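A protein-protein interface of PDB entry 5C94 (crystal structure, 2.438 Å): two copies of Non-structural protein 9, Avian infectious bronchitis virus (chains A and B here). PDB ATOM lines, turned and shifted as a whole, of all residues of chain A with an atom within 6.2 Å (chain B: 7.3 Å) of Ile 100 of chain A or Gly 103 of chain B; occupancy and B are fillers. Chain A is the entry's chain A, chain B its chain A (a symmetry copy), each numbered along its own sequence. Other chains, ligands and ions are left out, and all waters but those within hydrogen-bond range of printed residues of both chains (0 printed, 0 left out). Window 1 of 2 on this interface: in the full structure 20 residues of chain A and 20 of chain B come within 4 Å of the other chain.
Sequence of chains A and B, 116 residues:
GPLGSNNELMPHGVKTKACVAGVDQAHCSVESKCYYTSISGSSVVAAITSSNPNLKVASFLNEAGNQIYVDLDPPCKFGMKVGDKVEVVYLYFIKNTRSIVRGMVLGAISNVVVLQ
The backbone NH of Met 104 of chain B sits close to the backbone carbonyl oxygen of Gly 103 of chain A (3.4 Å).
The backbone NH of Met 104 of chain A sits close to the backbone carbonyl oxygen of Gly 103 of chain B, 3.4 Å away.
NE of Arg 102 of chain B is in hydrogen-bond range of O of Thr 97 of chain B, 3.0 Å away.
Among the printed residues, merely in contact across the chains: Gly 107 of chain A with Met 104 of chain B, Met 104 of chain A with Gly 107 of chain B, Ile 100 of chain A with Ser 99 of chain B, Ser 99 of chain A with Ile 100 of chain B, Ile 100 of chain A with Gly 103 of chain B, Gly 103 of chain A with Ile 100 of chain B, Gly 103 of chain A with Gly 103 of chain B, Leu 3 of chain A with Arg 102 of chain B, Gly 107 of chain A with Ala 108 of chain B, Ala 108 of chain A with Gly 107 of chain B, Gly 107 of chain A with Gly 107 of chain B, Ser 99 of chain A with Ser 99 of chain B and Leu 3 of chain A with Phe 93 of chain B.
Of the printed residues of chain B, Ser 99 of chain A touches Ser 99 (3.8 Å) and Ile 100 (3.3 Å).
Printed residues of chain B within 4 Å of Gly 107 of chain A: Met 104 (3.2 Å), Gly 107 (3.4 Å) and Ala 108 (3.4 Å).
Of the printed residues of chain B, Ala 108 of chain A touches Gly 107 (3.4 Å).
Printed residues of chain A within 4 Å of Ile 100 of chain B: Ser 99 (3.3 Å) and Gly 103 (3.3 Å).
Printed residues of chain A within 4 Å of Gly 103 of chain B: Ile 100 (3.3 Å), Gly 103 (3.4 Å) and Met 104 (3.2 Å).
Val 105 of chain B touches none of the printed residues of chain A.
Leu 106 of chain B touches none of the printed residues of chain A.
Printed residues of chain A within 4 Å of Ala 108 of chain B: Gly 107.
Of the 15 printed residues of chain B, 8 touch a printed residue of chain A.
Of the 15 printed residues of chain A, 7 touch a printed residue of chain B.
Hydrophobic or aromatic side chains of chain A that line the printed part of chain B: Leu 3, Ile 100, Met 104 and Ala 108.
Among the printed residues, no Asp or Glu carboxylate lies within 4 Å of a Lys or Arg side-chain nitrogen of the other chain.
Ser 99 of chain A touches its own counterpart, Ser 99 of chain B.
Ile 100 of chain A touches Gly 103 of chain B, and with the chains exchanged Gly 103 of chain A touches Ile 100 of chain B.
Gly 103 of chain B touches its own counterpart, Gly 103 of chain A.
Met 104 of chain A touches Gly 107 of chain B, and with the chains exchanged Gly 107 of chain A touches Met 104 of chain B.
11 positions are printed for both chains.
Of the 15 pairs that touch across the chains among the printed residues, 13 have their exchanged pair printed and touching as well.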
ATOM      1  N   LEU A   3      14.563 -31.418  25.568  1.00  0.00           N
ATOM      2  CA  LEU A   3      15.945 -30.927  25.511  1.00  0.00           C
ATOM      3  C   LEU A   3      16.870 -31.782  24.628  1.00  0.00           C
ATOM      4  O   LEU A   3      18.079 -31.532  24.569  1.00  0.00           O
ATOM      5  CB  LEU A   3      16.542 -30.811  26.922  1.00  0.00           C
ATOM      6  CG  LEU A   3      15.730 -30.096  28.007  1.00  0.00           C
ATOM      7  CD1 LEU A   3      16.507 -30.052  29.317  1.00  0.00           C
ATOM      8  CD2 LEU A   3      15.356 -28.693  27.562  1.00  0.00           C
ATOM      9  N   LEU A   9      17.909 -33.432  32.088  1.00  0.00           N
ATOM     10  CA  LEU A   9      17.417 -32.866  33.342  1.00  0.00           C
ATOM     11  C   LEU A   9      17.209 -31.358  33.191  1.00  0.00           C
ATOM     12  O   LEU A   9      18.164 -30.612  32.972  1.00  0.00           O
ATOM     13  CB  LEU A   9      18.360 -33.170  34.502  1.00  0.00           C
ATOM     14  CG  LEU A   9      17.675 -33.441  35.831  1.00  0.00           C
ATOM     15  CD1 LEU A   9      16.457 -34.349  35.637  1.00  0.00           C
ATOM     16  CD2 LEU A   9      18.683 -34.079  36.776  1.00  0.00           C
ATOM     17  N   MET A  10      15.959 -30.906  33.301  1.00  0.00           N
ATOM     18  CA  MET A  10      15.682 -29.498  33.033  1.00  0.00           C
ATOM     19  C   MET A  10      15.784 -28.624  34.276  1.00  0.00           C
ATOM     20  O   MET A  10      15.172 -28.898  35.316  1.00  0.00           O
ATOM     21  CB  MET A  10      14.306 -29.286  32.392  1.00  0.00           C
ATOM     22  CG  MET A  10      14.098 -27.816  32.008  1.00  0.00           C
ATOM     23  SD  MET A  10      12.847 -27.456  30.769  1.00  0.00           S
ATOM     24  CE  MET A  10      11.533 -26.876  31.843  1.00  0.00           C
ATOM     25  N   PRO A  11      16.581 -27.565  34.157  1.00  0.00           N
ATOM     26  CA  PRO A  11      16.810 -26.556  35.195  1.00  0.00           C
ATOM     27  C   PRO A  11      15.663 -25.540  35.271  1.00  0.00           C
ATOM     28  O   PRO A  11      15.048 -25.202  34.258  1.00  0.00           O
ATOM     29  CB  PRO A  11      18.123 -25.902  34.763  1.00  0.00           C
ATOM     30  CG  PRO A  11      18.237 -26.190  33.287  1.00  0.00           C
ATOM     31  CD  PRO A  11      17.494 -27.435  33.006  1.00  0.00           C
ATOM     32  N   THR A  97      30.258 -26.339  34.870  1.00  0.00           N
ATOM     33  CA  THR A  97      28.837 -26.083  34.830  1.00  0.00           C
ATOM     34  C   THR A  97      28.306 -26.644  33.514  1.00  0.00           C
ATOM     35  O   THR A  97      28.980 -26.567  32.489  1.00  0.00           O
ATOM     36  CB  THR A  97      28.542 -24.577  34.967  1.00  0.00           C
ATOM     37  OG1 THR A  97      28.876 -24.157  36.295  1.00  0.00           O
ATOM     38  CG2 THR A  97      27.062 -24.290  34.717  1.00  0.00           C
ATOM     39  N   ARG A  98      27.126 -27.255  33.555  1.00  0.00           N
ATOM     40  CA  ARG A  98      26.492 -27.777  32.347  1.00  0.00           C
ATOM     41  C   ARG A  98      26.210 -26.647  31.350  1.00  0.00           C
ATOM     42  O   ARG A  98      25.917 -25.510  31.750  1.00  0.00           O
ATOM     43  CB  ARG A  98      25.191 -28.494  32.693  1.00  0.00           C
ATOM     44  CG  ARG A  98      25.379 -29.813  33.425  1.00  0.00           C
ATOM     45  CD  ARG A  98      24.225 -30.774  33.099  1.00  0.00           C
ATOM     46  NE  ARG A  98      22.980 -30.442  33.784  1.00  0.00           N
ATOM     47  CZ  ARG A  98      21.761 -30.551  33.252  1.00  0.00           C
ATOM     48  NH1 ARG A  98      21.597 -30.956  32.000  1.00  0.00           N
ATOM     49  NH2 ARG A  98      20.697 -30.232  33.976  1.00  0.00           N
ATOM     50  N   SER A  99      26.284 -26.966  30.059  1.00  0.00           N
ATOM     51  CA  SER A  99      26.115 -25.973  28.999  1.00  0.00           C
ATOM     52  C   SER A  99      24.746 -25.295  29.039  1.00  0.00           C
ATOM     53  O   SER A  99      24.627 -24.085  28.809  1.00  0.00           O
ATOM     54  CB  SER A  99      26.319 -26.623  27.632  1.00  0.00           C
ATOM     55  OG  SER A  99      27.662 -27.016  27.452  1.00  0.00           O
ATOM     56  N   ILE A 100      23.712 -26.081  29.327  1.00  0.00           N
ATOM     57  CA  ILE A 100      22.366 -25.551  29.357  1.00  0.00           C
ATOM     58  C   ILE A 100      22.236 -24.595  30.545  1.00  0.00           C
ATOM     59  O   ILE A 100      21.551 -23.576  30.462  1.00  0.00           O
ATOM     60  CB  ILE A 100      21.312 -26.694  29.407  1.00  0.00           C
ATOM     61  CG1 ILE A 100      19.908 -26.144  29.195  1.00  0.00           C
ATOM     62  CG2 ILE A 100      21.384 -27.495  30.701  1.00  0.00           C
ATOM     63  CD1 ILE A 100      18.851 -27.242  29.038  1.00  0.00           C
ATOM     64  N   VAL A 101      22.941 -24.895  31.631  1.00  0.00           N
ATOM     65  CA  VAL A 101      22.873 -24.053  32.811  1.00  0.00           C
ATOM     66  C   VAL A 101      23.649 -22.758  32.579  1.00  0.00           C
ATOM     67  O   VAL A 101      23.216 -21.685  33.019  1.00  0.00           O
ATOM     68  CB  VAL A 101      23.388 -24.794  34.061  1.00  0.00           C
ATOM     69  CG1 VAL A 101      23.445 -23.868  35.248  1.00  0.00           C
ATOM     70  CG2 VAL A 101      22.475 -25.978  34.384  1.00  0.00           C
ATOM     71  N   ARG A 102      24.777 -22.846  31.871  1.00  0.00           N
ATOM     72  CA  ARG A 102      25.500 -21.636  31.461  1.00  0.00           C
ATOM     73  C   ARG A 102      24.611 -20.727  30.615  1.00  0.00           C
ATOM     74  O   ARG A 102      24.589 -19.513  30.796  1.00  0.00           O
ATOM     75  CB  ARG A 102      26.761 -21.981  30.666  1.00  0.00           C
ATOM     76  CG  ARG A 102      27.823 -22.722  31.460  1.00  0.00           C
ATOM     77  CD  ARG A 102      29.038 -23.066  30.606  1.00  0.00           C
ATOM     78  NE  ARG A 102      29.907 -23.995  31.317  1.00  0.00           N
ATOM     79  CZ  ARG A 102      31.083 -23.665  31.844  1.00  0.00           C
ATOM     80  NH1 ARG A 102      31.552 -22.431  31.716  1.00  0.00           N
ATOM     81  NH2 ARG A 102      31.802 -24.574  32.483  1.00  0.00           N
ATOM     82  N   GLY A 103      23.891 -21.329  29.674  1.00  0.00           N
ATOM     83  CA  GLY A 103      23.011 -20.582  28.801  1.00  0.00           C
ATOM     84  C   GLY A 103      21.905 -19.906  29.587  1.00  0.00           C
ATOM     85  O   GLY A 103      21.534 -18.760  29.285  1.00  0.00           O
ATOM     86  N   MET A 104      21.388 -20.593  30.598  1.00  0.00           N
ATOM     87  CA  MET A 104      20.312 -20.031  31.394  1.00  0.00           C
ATOM     88  C   MET A 104      20.712 -18.723  32.060  1.00  0.00           C
ATOM     89  O   MET A 104      19.931 -17.777  32.084  1.00  0.00           O
ATOM     90  CB  MET A 104      19.852 -21.033  32.435  1.00  0.00           C
ATOM     91  CG  MET A 104      19.026 -22.138  31.835  1.00  0.00           C
ATOM     92  SD  MET A 104      18.155 -23.012  33.123  1.00  0.00           S
ATOM     93  CE  MET A 104      17.611 -21.643  34.137  1.00  0.00           C
ATOM     94  N   VAL A 105      21.933 -18.669  32.587  1.00  0.00           N
ATOM     95  CA  VAL A 105      22.467 -17.431  33.135  1.00  0.00           C
ATOM     96  C   VAL A 105      22.566 -16.360  32.046  1.00  0.00           C
ATOM     97  O   VAL A 105      22.183 -15.209  32.267  1.00  0.00           O
ATOM     98  CB  VAL A 105      23.863 -17.627  33.763  1.00  0.00           C
ATOM     99  CG1 VAL A 105      24.432 -16.280  34.228  1.00  0.00           C
ATOM    100  CG2 VAL A 105      23.805 -18.599  34.926  1.00  0.00           C
ATOM    101  N   GLY A 107      20.923 -16.147  29.275  1.00  0.00           N
ATOM    102  CA  GLY A 107      19.573 -15.777  28.913  1.00  0.00           C
ATOM    103  C   GLY A 107      18.980 -14.817  29.930  1.00  0.00           C
ATOM    104  O   GLY A 107      18.316 -13.856  29.552  1.00  0.00           O
ATOM    105  N   ALA A 108      19.228 -15.068  31.216  1.00  0.00           N
ATOM    106  CA  ALA A 108      18.608 -14.276  32.282  1.00  0.00           C
ATOM    107  C   ALA A 108      19.122 -12.843  32.294  1.00  0.00           C
ATOM    108  O   ALA A 108      18.402 -11.927  32.686  1.00  0.00           O
ATOM    109  CB  ALA A 108      18.842 -14.915  33.642  1.00  0.00           C
ATOM    110  N   VAL B  14      18.867 -12.556  23.094  1.00  0.00           N
ATOM    111  CA  VAL B  14      17.729 -13.373  22.715  1.00  0.00           C
ATOM    112  C   VAL B  14      16.709 -12.427  22.125  1.00  0.00           C
ATOM    113  O   VAL B  14      16.298 -11.474  22.770  1.00  0.00           O
ATOM    114  CB  VAL B  14      17.106 -14.140  23.905  1.00  0.00           C
ATOM    115  CG1 VAL B  14      15.818 -14.828  23.477  1.00  0.00           C
ATOM    116  CG2 VAL B  14      18.099 -15.144  24.503  1.00  0.00           C
ATOM    117  N   PHE B  93      11.895 -26.511  21.263  1.00  0.00           N
ATOM    118  CA  PHE B  93      13.216 -26.220  20.747  1.00  0.00           C
ATOM    119  C   PHE B  93      13.324 -26.856  19.387  1.00  0.00           C
ATOM    120  O   PHE B  93      12.671 -27.850  19.085  1.00  0.00           O
ATOM    121  CB  PHE B  93      14.322 -26.731  21.668  1.00  0.00           C
ATOM    122  CG  PHE B  93      14.408 -25.993  22.965  1.00  0.00           C
ATOM    123  CD1 PHE B  93      14.901 -24.693  23.008  1.00  0.00           C
ATOM    124  CD2 PHE B  93      13.972 -26.589  24.142  1.00  0.00           C
ATOM    125  CE1 PHE B  93      14.977 -24.006  24.208  1.00  0.00           C
ATOM    126  CE2 PHE B  93      14.044 -25.916  25.349  1.00  0.00           C
ATOM    127  CZ  PHE B  93      14.544 -24.620  25.386  1.00  0.00           C
ATOM    128  N   THR B  97      19.363 -28.126  18.488  1.00  0.00           N
ATOM    129  CA  THR B  97      19.822 -26.856  19.001  1.00  0.00           C
ATOM    130  C   THR B  97      20.889 -27.145  20.054  1.00  0.00           C
ATOM    131  O   THR B  97      20.777 -28.114  20.802  1.00  0.00           O
ATOM    132  CB  THR B  97      18.652 -26.040  19.585  1.00  0.00           C
ATOM    133  OG1 THR B  97      17.794 -25.628  18.515  1.00  0.00           O
ATOM    134  CG2 THR B  97      19.167 -24.798  20.310  1.00  0.00           C
ATOM    135  N   ARG B  98      21.945 -26.338  20.074  1.00  0.00           N
ATOM    136  CA  ARG B  98      22.999 -26.481  21.075  1.00  0.00           C
ATOM    137  C   ARG B  98      22.438 -26.276  22.487  1.00  0.00           C
ATOM    138  O   ARG B  98      21.511 -25.477  22.687  1.00  0.00           O
ATOM    139  CB  ARG B  98      24.122 -25.482  20.817  1.00  0.00           C
ATOM    140  CG  ARG B  98      24.956 -25.783  19.582  1.00  0.00           C
ATOM    141  CD  ARG B  98      26.391 -25.270  19.769  1.00  0.00           C
ATOM    142  NE  ARG B  98      26.514 -23.821  19.637  1.00  0.00           N
ATOM    143  CZ  ARG B  98      27.315 -23.050  20.374  1.00  0.00           C
ATOM    144  NH1 ARG B  98      28.062 -23.569  21.340  1.00  0.00           N
ATOM    145  NH2 ARG B  98      27.354 -21.743  20.155  1.00  0.00           N
ATOM    146  N   SER B  99      23.011 -26.982  23.460  1.00  0.00           N
ATOM    147  CA  SER B  99      22.529 -26.943  24.840  1.00  0.00           C
ATOM    148  C   SER B  99      22.587 -25.542  25.445  1.00  0.00           C
ATOM    149  O   SER B  99      21.681 -25.127  26.179  1.00  0.00           O
ATOM    150  CB  SER B  99      23.341 -27.904  25.707  1.00  0.00           C
ATOM    151  OG  SER B  99      23.092 -29.246  25.349  1.00  0.00           O
ATOM    152  N   ILE B 100      23.658 -24.815  25.139  1.00  0.00           N
ATOM    153  CA  ILE B 100      23.832 -23.487  25.685  1.00  0.00           C
ATOM    154  C   ILE B 100      22.774 -22.560  25.082  1.00  0.00           C
ATOM    155  O   ILE B 100      22.255 -21.671  25.757  1.00  0.00           O
ATOM    156  CB  ILE B 100      25.276 -22.963  25.443  1.00  0.00           C
ATOM    157  CG1 ILE B 100      25.524 -21.679  26.225  1.00  0.00           C
ATOM    158  CG2 ILE B 100      25.580 -22.757  23.965  1.00  0.00           C
ATOM    159  CD1 ILE B 100      26.987 -21.224  26.182  1.00  0.00           C
ATOM    160  N   VAL B 101      22.413 -22.806  23.827  1.00  0.00           N
ATOM    161  CA  VAL B 101      21.425 -21.973  23.167  1.00  0.00           C
ATOM    162  C   VAL B 101      20.030 -22.286  23.703  1.00  0.00           C
ATOM    163  O   VAL B 101      19.211 -21.374  23.879  1.00  0.00           O
ATOM    164  CB  VAL B 101      21.482 -22.138  21.635  1.00  0.00           C
ATOM    165  CG1 VAL B 101      20.363 -21.381  20.971  1.00  0.00           C
ATOM    166  CG2 VAL B 101      22.824 -21.635  21.101  1.00  0.00           C
ATOM    167  N   ARG B 102      19.762 -23.562  23.987  1.00  0.00           N
ATOM    168  CA  ARG B 102      18.511 -23.933  24.658  1.00  0.00           C
ATOM    169  C   ARG B 102      18.380 -23.227  26.006  1.00  0.00           C
ATOM    170  O   ARG B 102      17.318 -22.722  26.358  1.00  0.00           O
ATOM    171  CB  ARG B 102      18.420 -25.445  24.876  1.00  0.00           C
ATOM    172  CG  ARG B 102      18.342 -26.263  23.599  1.00  0.00           C
ATOM    173  CD  ARG B 102      18.288 -27.760  23.882  1.00  0.00           C
ATOM    174  NE  ARG B 102      18.480 -28.512  22.648  1.00  0.00           N
ATOM    175  CZ  ARG B 102      17.514 -29.175  22.019  1.00  0.00           C
ATOM    176  NH1 ARG B 102      16.286 -29.206  22.519  1.00  0.00           N
ATOM    177  NH2 ARG B 102      17.777 -29.824  20.895  1.00  0.00           N
ATOM    178  N   GLY B 103      19.472 -23.213  26.764  1.00  0.00           N
ATOM    179  CA  GLY B 103      19.481 -22.580  28.065  1.00  0.00           C
ATOM    180  C   GLY B 103      19.221 -21.091  27.951  1.00  0.00           C
ATOM    181  O   GLY B 103      18.506 -20.516  28.787  1.00  0.00           O
ATOM    182  N   MET B 104      19.778 -20.467  26.921  1.00  0.00           N
ATOM    183  CA  MET B 104      19.597 -19.038  26.742  1.00  0.00           C
ATOM    184  C   MET B 104      18.131 -18.656  26.601  1.00  0.00           C
ATOM    185  O   MET B 104      17.692 -17.666  27.179  1.00  0.00           O
ATOM    186  CB  MET B 104      20.386 -18.556  25.540  1.00  0.00           C
ATOM    187  CG  MET B 104      21.862 -18.482  25.820  1.00  0.00           C
ATOM    188  SD  MET B 104      22.670 -17.507  24.563  1.00  0.00           S
ATOM    189  CE  MET B 104      21.503 -16.163  24.391  1.00  0.00           C
ATOM    190  N   VAL B 105      17.378 -19.450  25.845  1.00  0.00           N
ATOM    191  CA  VAL B 105      15.939 -19.254  25.742  1.00  0.00           C
ATOM    192  C   VAL B 105      15.274 -19.427  27.109  1.00  0.00           C
ATOM    193  O   VAL B 105      14.423 -18.622  27.495  1.00  0.00           O
ATOM    194  CB  VAL B 105      15.287 -20.238  24.748  1.00  0.00           C
ATOM    195  CG1 VAL B 105      13.762 -20.069  24.753  1.00  0.00           C
ATOM    196  CG2 VAL B 105      15.831 -20.035  23.346  1.00  0.00           C
ATOM    197  N   LEU B 106      15.655 -20.475  27.837  1.00  0.00           N
ATOM    198  CA  LEU B 106      15.041 -20.739  29.139  1.00  0.00           C
ATOM    199  C   LEU B 106      15.349 -19.596  30.093  1.00  0.00           C
ATOM    200  O   LEU B 106      14.484 -19.163  30.860  1.00  0.00           O
ATOM    201  CB  LEU B 106      15.522 -22.069  29.735  1.00  0.00           C
ATOM    202  CG  LEU B 106      15.078 -23.346  29.018  1.00  0.00           C
ATOM    203  CD1 LEU B 106      15.710 -24.569  29.670  1.00  0.00           C
ATOM    204  CD2 LEU B 106      13.557 -23.477  28.993  1.00  0.00           C
ATOM    205  N   GLY B 107      16.588 -19.119  30.043  1.00  0.00           N
ATOM    206  CA  GLY B 107      17.002 -18.004  30.865  1.00  0.00           C
ATOM    207  C   GLY B 107      16.202 -16.757  30.533  1.00  0.00           C
ATOM    208  O   GLY B 107      15.800 -16.028  31.436  1.00  0.00           O
ATOM    209  N   ALA B 108      15.961 -16.517  29.244  1.00  0.00           N
ATOM    210  CA  ALA B 108      15.303 -15.282  28.806  1.00  0.00           C
ATOM    211  C   ALA B 108      13.850 -15.226  29.257  1.00  0.00           C
ATOM    212  O   ALA B 108      13.310 -14.145  29.484  1.00  0.00           O
ATOM    213  CB  ALA B 108      15.376 -15.131  27.295  1.00  0.00           C
ATOM    214  N   ILE B 109      13.217 -16.384  29.405  1.00  0.00           N
ATOM    215  CA  ILE B 109      11.791 -16.416  29.752  1.00  0.00           C
ATOM    216  C   ILE B 109      11.561 -16.688  31.235  1.00  0.00           C
ATOM    217  O   ILE B 109      10.427 -16.644  31.703  1.00  0.00           O
ATOM    218  CB  ILE B 109      11.028 -17.480  28.927  1.00  0.00           C
ATOM    219  CG1 ILE B 109      11.511 -18.887  29.303  1.00  0.00           C
ATOM    220  CG2 ILE B 109      11.184 -17.214  27.421  1.00  0.00           C
ATOM    221  CD1 ILE B 109      10.805 -19.991  28.575  1.00  0.00           C
